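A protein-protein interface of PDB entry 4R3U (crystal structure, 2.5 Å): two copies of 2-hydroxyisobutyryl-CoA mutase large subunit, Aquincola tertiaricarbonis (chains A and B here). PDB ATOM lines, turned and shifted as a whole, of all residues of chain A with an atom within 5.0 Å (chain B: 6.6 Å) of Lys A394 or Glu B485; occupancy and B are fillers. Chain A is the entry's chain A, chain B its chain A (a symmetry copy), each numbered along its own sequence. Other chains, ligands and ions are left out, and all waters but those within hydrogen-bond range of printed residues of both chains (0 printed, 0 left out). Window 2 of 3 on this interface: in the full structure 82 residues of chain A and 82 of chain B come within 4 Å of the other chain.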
ATOM      1  N   TYR A 116     -18.540  -4.386   2.809  1.00  0.00           N
ATOM      2  CA  TYR A 116     -17.538  -4.932   3.720  1.00  0.00           C
ATOM      3  C   TYR A 116     -18.169  -6.000   4.633  1.00  0.00           C
ATOM      4  O   TYR A 116     -17.621  -7.105   4.785  1.00  0.00           O
ATOM      5  CB  TYR A 116     -16.922  -3.823   4.587  1.00  0.00           C
ATOM      6  CG  TYR A 116     -16.025  -4.374   5.663  1.00  0.00           C
ATOM      7  CD1 TYR A 116     -14.719  -4.770   5.375  1.00  0.00           C
ATOM      8  CD2 TYR A 116     -16.503  -4.581   6.960  1.00  0.00           C
ATOM      9  CE1 TYR A 116     -13.896  -5.322   6.359  1.00  0.00           C
ATOM     10  CE2 TYR A 116     -15.698  -5.159   7.944  1.00  0.00           C
ATOM     11  CZ  TYR A 116     -14.388  -5.506   7.642  1.00  0.00           C
ATOM     12  OH  TYR A 116     -13.572  -6.031   8.607  1.00  0.00           O
ATOM     13  N   GLN A 120     -17.661 -10.043   4.980  1.00  0.00           N
ATOM     14  CA  GLN A 120     -17.321 -10.640   6.276  1.00  0.00           C
ATOM     15  C   GLN A 120     -18.326 -11.686   6.784  1.00  0.00           C
ATOM     16  O   GLN A 120     -18.064 -12.336   7.795  1.00  0.00           O
ATOM     17  CB  GLN A 120     -17.026  -9.581   7.347  1.00  0.00           C
ATOM     18  CG  GLN A 120     -15.809  -8.686   7.066  1.00  0.00           C
ATOM     19  CD  GLN A 120     -14.593  -9.343   6.444  1.00  0.00           C
ATOM     20  OE1 GLN A 120     -14.161 -10.434   6.788  1.00  0.00           O
ATOM     21  NE2 GLN A 120     -14.011  -8.673   5.515  1.00  0.00           N
ATOM     22  N   GLU A 390     -14.407  -1.239  11.058  1.00  0.00           N
ATOM     23  CA  GLU A 390     -14.530  -2.467  10.300  1.00  0.00           C
ATOM     24  C   GLU A 390     -14.088  -3.656  11.149  1.00  0.00           C
ATOM     25  O   GLU A 390     -14.851  -4.600  11.269  1.00  0.00           O
ATOM     26  CB  GLU A 390     -13.706  -2.363   9.027  1.00  0.00           C
ATOM     27  CG  GLU A 390     -14.332  -1.436   8.011  1.00  0.00           C
ATOM     28  CD  GLU A 390     -13.641  -1.431   6.667  1.00  0.00           C
ATOM     29  OE1 GLU A 390     -12.420  -1.700   6.633  1.00  0.00           O
ATOM     30  OE2 GLU A 390     -14.315  -1.148   5.651  1.00  0.00           O
ATOM     31  N   ASP A 391     -12.922  -3.569  11.812  1.00  0.00           N
ATOM     32  CA  ASP A 391     -12.380  -4.638  12.675  1.00  0.00           C
ATOM     33  C   ASP A 391     -13.309  -5.036  13.814  1.00  0.00           C
ATOM     34  O   ASP A 391     -13.440  -6.210  14.101  1.00  0.00           O
ATOM     35  CB  ASP A 391     -10.993  -4.268  13.238  1.00  0.00           C
ATOM     36  CG  ASP A 391      -9.823  -4.294  12.273  1.00  0.00           C
ATOM     37  OD1 ASP A 391      -9.926  -4.980  11.222  1.00  0.00           O
ATOM     38  OD2 ASP A 391      -8.769  -3.683  12.599  1.00  0.00           O
ATOM     39  N   ALA A 392     -13.937  -4.051  14.460  1.00  0.00           N
ATOM     40  CA  ALA A 392     -14.878  -4.225  15.555  1.00  0.00           C
ATOM     41  C   ALA A 392     -16.122  -4.983  15.056  1.00  0.00           C
ATOM     42  O   ALA A 392     -16.554  -5.936  15.706  1.00  0.00           O
ATOM     43  CB  ALA A 392     -15.263  -2.872  16.121  1.00  0.00           C
ATOM     44  N   MET A 393     -16.653  -4.606  13.880  1.00  0.00           N
ATOM     45  CA  MET A 393     -17.783  -5.288  13.258  1.00  0.00           C
ATOM     46  C   MET A 393     -17.434  -6.672  12.815  1.00  0.00           C
ATOM     47  O   MET A 393     -18.220  -7.591  13.036  1.00  0.00           O
ATOM     48  CB  MET A 393     -18.417  -4.452  12.134  1.00  0.00           C
ATOM     49  CG  MET A 393     -19.231  -3.258  12.648  1.00  0.00           C
ATOM     50  SD  MET A 393     -20.704  -3.688  13.650  1.00  0.00           S
ATOM     51  CE  MET A 393     -20.033  -3.691  15.333  1.00  0.00           C
ATOM     52  N   LYS A 394     -16.226  -6.856  12.266  1.00  0.00           N
ATOM     53  CA  LYS A 394     -15.679  -8.158  11.841  1.00  0.00           C
ATOM     54  C   LYS A 394     -15.659  -9.112  13.047  1.00  0.00           C
ATOM     55  O   LYS A 394     -16.155 -10.231  12.937  1.00  0.00           O
ATOM     56  CB  LYS A 394     -14.281  -7.967  11.279  1.00  0.00           C
ATOM     57  CG  LYS A 394     -13.913  -8.957  10.176  1.00  0.00           C
ATOM     58  CD  LYS A 394     -12.420  -9.292  10.090  1.00  0.00           C
ATOM     59  CE  LYS A 394     -11.431  -8.164  10.092  1.00  0.00           C
ATOM     60  NZ  LYS A 394     -10.036  -8.672   9.990  1.00  0.00           N
ATOM     61  N   MET A 395     -15.177  -8.634  14.230  1.00  0.00           N
ATOM     62  CA  MET A 395     -15.111  -9.418  15.472  1.00  0.00           C
ATOM     63  C   MET A 395     -16.514  -9.807  15.951  1.00  0.00           C
ATOM     64  O   MET A 395     -16.720 -10.958  16.392  1.00  0.00           O
ATOM     65  CB  MET A 395     -14.324  -8.676  16.537  1.00  0.00           C
ATOM     66  CG  MET A 395     -14.242  -9.406  17.906  1.00  0.00           C
ATOM     67  SD  MET A 395     -13.420 -11.016  17.865  1.00  0.00           S
ATOM     68  CE  MET A 395     -11.744 -10.545  17.342  1.00  0.00           C
ATOM     69  N   ALA A 396     -17.494  -8.875  15.803  1.00  0.00           N
ATOM     70  CA  ALA A 396     -18.890  -9.093  16.157  1.00  0.00           C
ATOM     71  C   ALA A 396     -19.495 -10.176  15.284  1.00  0.00           C
ATOM     72  O   ALA A 396     -20.234 -11.006  15.794  1.00  0.00           O
ATOM     73  CB  ALA A 396     -19.664  -7.801  16.040  1.00  0.00           C
ATOM     74  N   LEU A 397     -19.129 -10.226  13.992  1.00  0.00           N
ATOM     75  CA  LEU A 397     -19.593 -11.278  13.082  1.00  0.00           C
ATOM     76  C   LEU A 397     -18.921 -12.627  13.399  1.00  0.00           C
ATOM     77  O   LEU A 397     -19.620 -13.633  13.432  1.00  0.00           O
ATOM     78  CB  LEU A 397     -19.383 -10.880  11.610  1.00  0.00           C
ATOM     79  CG  LEU A 397     -20.353  -9.836  11.070  1.00  0.00           C
ATOM     80  CD1 LEU A 397     -19.794  -9.157   9.825  1.00  0.00           C
ATOM     81  CD2 LEU A 397     -21.724 -10.452  10.802  1.00  0.00           C
ATOM     82  N   ARG A 398     -17.595 -12.643  13.702  1.00  0.00           N
ATOM     83  CA  ARG A 398     -16.871 -13.870  14.047  1.00  0.00           C
ATOM     84  C   ARG A 398     -17.464 -14.524  15.292  1.00  0.00           C
ATOM     85  O   ARG A 398     -17.529 -15.759  15.373  1.00  0.00           O
ATOM     86  CB  ARG A 398     -15.356 -13.620  14.205  1.00  0.00           C
ATOM     87  CG  ARG A 398     -14.615 -13.182  12.940  1.00  0.00           C
ATOM     88  CD  ARG A 398     -14.546 -14.223  11.837  1.00  0.00           C
ATOM     89  NE  ARG A 398     -13.975 -13.644  10.624  1.00  0.00           N
ATOM     90  CZ  ARG A 398     -14.684 -13.190   9.591  1.00  0.00           C
ATOM     91  NH1 ARG A 398     -16.008 -13.254   9.601  1.00  0.00           N
ATOM     92  NH2 ARG A 398     -14.072 -12.669   8.537  1.00  0.00           N
ATOM     93  N   PRO B 352      -4.480 -18.262  12.789  1.00  0.00           N
ATOM     94  CA  PRO B 352      -5.160 -17.180  12.049  1.00  0.00           C
ATOM     95  C   PRO B 352      -6.277 -16.560  12.888  1.00  0.00           C
ATOM     96  O   PRO B 352      -6.941 -17.272  13.670  1.00  0.00           O
ATOM     97  CB  PRO B 352      -5.729 -17.890  10.815  1.00  0.00           C
ATOM     98  CG  PRO B 352      -5.822 -19.293  11.172  1.00  0.00           C
ATOM     99  CD  PRO B 352      -4.722 -19.575  12.141  1.00  0.00           C
ATOM    100  N   GLN B 353      -6.454 -15.225  12.778  1.00  0.00           N
ATOM    101  CA  GLN B 353      -7.509 -14.479  13.473  1.00  0.00           C
ATOM    102  C   GLN B 353      -7.540 -14.786  14.973  1.00  0.00           C
ATOM    103  O   GLN B 353      -8.627 -14.912  15.567  1.00  0.00           O
ATOM    104  CB  GLN B 353      -8.875 -14.762  12.816  1.00  0.00           C
ATOM    105  CG  GLN B 353      -8.932 -14.405  11.339  1.00  0.00           C
ATOM    106  CD  GLN B 353     -10.337 -14.494  10.836  1.00  0.00           C
ATOM    107  OE1 GLN B 353     -10.625 -15.211   9.869  1.00  0.00           O
ATOM    108  NE2 GLN B 353     -11.215 -13.698  11.444  1.00  0.00           N
ATOM    109  N   VAL B 356     -10.125 -13.978  17.982  1.00  0.00           N
ATOM    110  CA  VAL B 356     -11.389 -14.713  17.936  1.00  0.00           C
ATOM    111  C   VAL B 356     -11.408 -15.844  19.003  1.00  0.00           C
ATOM    112  O   VAL B 356     -12.476 -16.226  19.473  1.00  0.00           O
ATOM    113  CB  VAL B 356     -11.631 -15.158  16.468  1.00  0.00           C
ATOM    114  CG1 VAL B 356     -11.501 -16.657  16.266  1.00  0.00           C
ATOM    115  CG2 VAL B 356     -12.935 -14.641  15.963  1.00  0.00           C
ATOM    116  N   GLY B 479     -11.550 -19.159  10.538  1.00  0.00           N
ATOM    117  CA  GLY B 479     -10.206 -18.658  10.288  1.00  0.00           C
ATOM    118  C   GLY B 479      -9.344 -19.664   9.558  1.00  0.00           C
ATOM    119  O   GLY B 479      -8.374 -19.274   8.900  1.00  0.00           O
ATOM    120  N   ARG B 482     -13.158 -21.643   7.059  1.00  0.00           N
ATOM    121  CA  ARG B 482     -14.336 -20.802   7.094  1.00  0.00           C
ATOM    122  C   ARG B 482     -13.886 -19.386   7.377  1.00  0.00           C
ATOM    123  O   ARG B 482     -13.097 -19.144   8.310  1.00  0.00           O
ATOM    124  CB  ARG B 482     -15.199 -21.284   8.265  1.00  0.00           C
ATOM    125  CG  ARG B 482     -16.660 -21.440   7.992  1.00  0.00           C
ATOM    126  CD  ARG B 482     -17.053 -22.548   7.027  1.00  0.00           C
ATOM    127  NE  ARG B 482     -18.498 -22.489   6.788  1.00  0.00           N
ATOM    128  CZ  ARG B 482     -19.145 -21.496   6.163  1.00  0.00           C
ATOM    129  NH1 ARG B 482     -20.462 -21.538   6.024  1.00  0.00           N
ATOM    130  NH2 ARG B 482     -18.475 -20.457   5.679  1.00  0.00           N
ATOM    131  N   PHE B 483     -14.402 -18.435   6.563  1.00  0.00           N
ATOM    132  CA  PHE B 483     -14.126 -17.001   6.672  1.00  0.00           C
ATOM    133  C   PHE B 483     -12.627 -16.742   6.705  1.00  0.00           C
ATOM    134  O   PHE B 483     -12.156 -15.902   7.476  1.00  0.00           O
ATOM    135  CB  PHE B 483     -14.898 -16.361   7.858  1.00  0.00           C
ATOM    136  CG  PHE B 483     -16.394 -16.588   7.823  1.00  0.00           C
ATOM    137  CD1 PHE B 483     -17.214 -15.812   7.022  1.00  0.00           C
ATOM    138  CD2 PHE B 483     -16.975 -17.612   8.563  1.00  0.00           C
ATOM    139  CE1 PHE B 483     -18.577 -16.092   6.915  1.00  0.00           C
ATOM    140  CE2 PHE B 483     -18.345 -17.895   8.451  1.00  0.00           C
ATOM    141  CZ  PHE B 483     -19.135 -17.135   7.629  1.00  0.00           C
ATOM    142  N   VAL B 484     -11.876 -17.509   5.881  1.00  0.00           N
ATOM    143  CA  VAL B 484     -10.420 -17.452   5.763  1.00  0.00           C
ATOM    144  C   VAL B 484     -10.071 -16.080   5.187  1.00  0.00           C
ATOM    145  O   VAL B 484     -10.773 -15.590   4.286  1.00  0.00           O
ATOM    146  CB  VAL B 484      -9.825 -18.635   4.926  1.00  0.00           C
ATOM    147  CG1 VAL B 484      -8.312 -18.633   4.926  1.00  0.00           C
ATOM    148  CG2 VAL B 484     -10.334 -19.976   5.424  1.00  0.00           C
ATOM    149  N   GLU B 485      -9.045 -15.436   5.768  1.00  0.00           N
ATOM    150  CA  GLU B 485      -8.565 -14.101   5.422  1.00  0.00           C
ATOM    151  C   GLU B 485      -7.105 -14.135   5.046  1.00  0.00           C
ATOM    152  O   GLU B 485      -6.367 -14.912   5.628  1.00  0.00           O
ATOM    153  CB  GLU B 485      -8.691 -13.177   6.646  1.00  0.00           C
ATOM    154  CG  GLU B 485     -10.103 -12.707   6.948  1.00  0.00           C
ATOM    155  CD  GLU B 485     -10.274 -11.973   8.270  1.00  0.00           C
ATOM    156  OE1 GLU B 485      -9.328 -11.290   8.726  1.00  0.00           O
ATOM    157  OE2 GLU B 485     -11.368 -12.097   8.858  1.00  0.00           O
ATOM    158  N   ASN B 486      -6.654 -13.231   4.155  1.00  0.00           N
ATOM    159  CA  ASN B 486      -5.224 -13.126   3.881  1.00  0.00           C
ATOM    160  C   ASN B 486      -4.677 -11.916   4.691  1.00  0.00           C
ATOM    161  O   ASN B 486      -4.392 -10.847   4.129  1.00  0.00           O
ATOM    162  CB  ASN B 486      -4.922 -13.120   2.392  1.00  0.00           C
ATOM    163  CG  ASN B 486      -5.194 -14.468   1.754  1.00  0.00           C
ATOM    164  OD1 ASN B 486      -6.339 -14.833   1.451  1.00  0.00           O
ATOM    165  ND2 ASN B 486      -4.141 -15.245   1.547  1.00  0.00           N
ATOM    166  N   GLU B 487      -4.618 -12.103   6.061  1.00  0.00           N
ATOM    167  CA  GLU B 487      -4.138 -11.148   7.071  1.00  0.00           C
ATOM    168  C   GLU B 487      -2.642 -10.898   6.867  1.00  0.00           C
ATOM    169  O   GLU B 487      -1.827 -11.803   7.061  1.00  0.00           O
ATOM    170  CB  GLU B 487      -4.309 -11.709   8.496  1.00  0.00           C
ATOM    171  CG  GLU B 487      -5.684 -12.162   8.948  1.00  0.00           C
ATOM    172  CD  GLU B 487      -5.640 -12.851  10.305  1.00  0.00           C
ATOM    173  OE1 GLU B 487      -5.148 -13.999  10.380  1.00  0.00           O
ATOM    174  OE2 GLU B 487      -6.134 -12.256  11.288  1.00  0.00           O
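NZ of Lys A394 lies within salt-bridge range of OE1 of Glu B485.
The guanidinium group (NH2) of Arg A398 lies within salt-bridge range of the side-chain carboxylate (OE2) of Glu B485 (2.8 Å).
NE of Arg A398 sits close to NE2 of Gln B353.
The side-chain amide oxygen (OE1) of Gln B353 sits close to the backbone carbonyl oxygen (O) of Phe B483 (2.9 Å).
The side-chain amide oxygen (OE1) of Gln A120 is in hydrogen-bond range of the guanidinium group (NH2) of Arg A398, at 2.8 Å.
The side-chain carboxylate of Asp A391 lies within salt-bridge range of the side-chain amino group of Lys A394, 3.9 Å away.
The backbone NH of Gln B353 lies within hydrogen-bond range of the side-chain carboxylate of Glu B487, 3.0 Å away.
NE2 of Gln B353 sits at hydrogen-bond distance from OE2 of Glu B485 (3.0 Å).
CD1 of Phe B483 touches O of Gln A120, at 3.7 Å.
Gln A120 touches Glu B485.
Met A395 touches Val B356 (CE to N, 3.8 Å).
Val B356 touches Arg A398 (CG2 to CB, 3.2 Å).
Phe B483 touches Arg A398.
Lys A394 touches one residue of chain B.
Glu B485 touches just these residues of chain A: Gln A120, Lys A394 and Arg A398.
Of the printed residues of chain B, Arg A398 touches Gln B353 (2.9 Å), Val B356 (3.2 Å), Phe B483 (3.6 Å) and Glu B485 (2.8 Å).
Of the printed residues of chain A, Gln B353 touches Arg A398 (2.9 Å).
Printed residues of chain B within 4 Å of Gln A120: Phe B483 (3.7 Å) and Glu B485 (3.9 Å).
Printed residues of chain A within 4 Å of Phe B483: Gln A120 and Arg A398.
Glu A390 touches none of the printed residues of chain B.
Glu B487 touches none of the printed residues of chain A.
The nearest residue of chain B that does not touch Lys A394 is Gln B353 (4.8 Å).
The nearest printed residue of chain A that does not touch Glu B485 is Tyr A116 (6.5 Å).
Hydrophobic or aromatic side chains of chain A that line the printed part of chain B: Met A395.
Among the printed residues, Asp or Glu carboxylates within 4 Å of a Lys or Arg side-chain nitrogen of the other chain: Lys A394 with Glu B485 (3.0 Å) and Arg A398 with Glu B485 (2.8 Å).
No position is printed for both chains.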
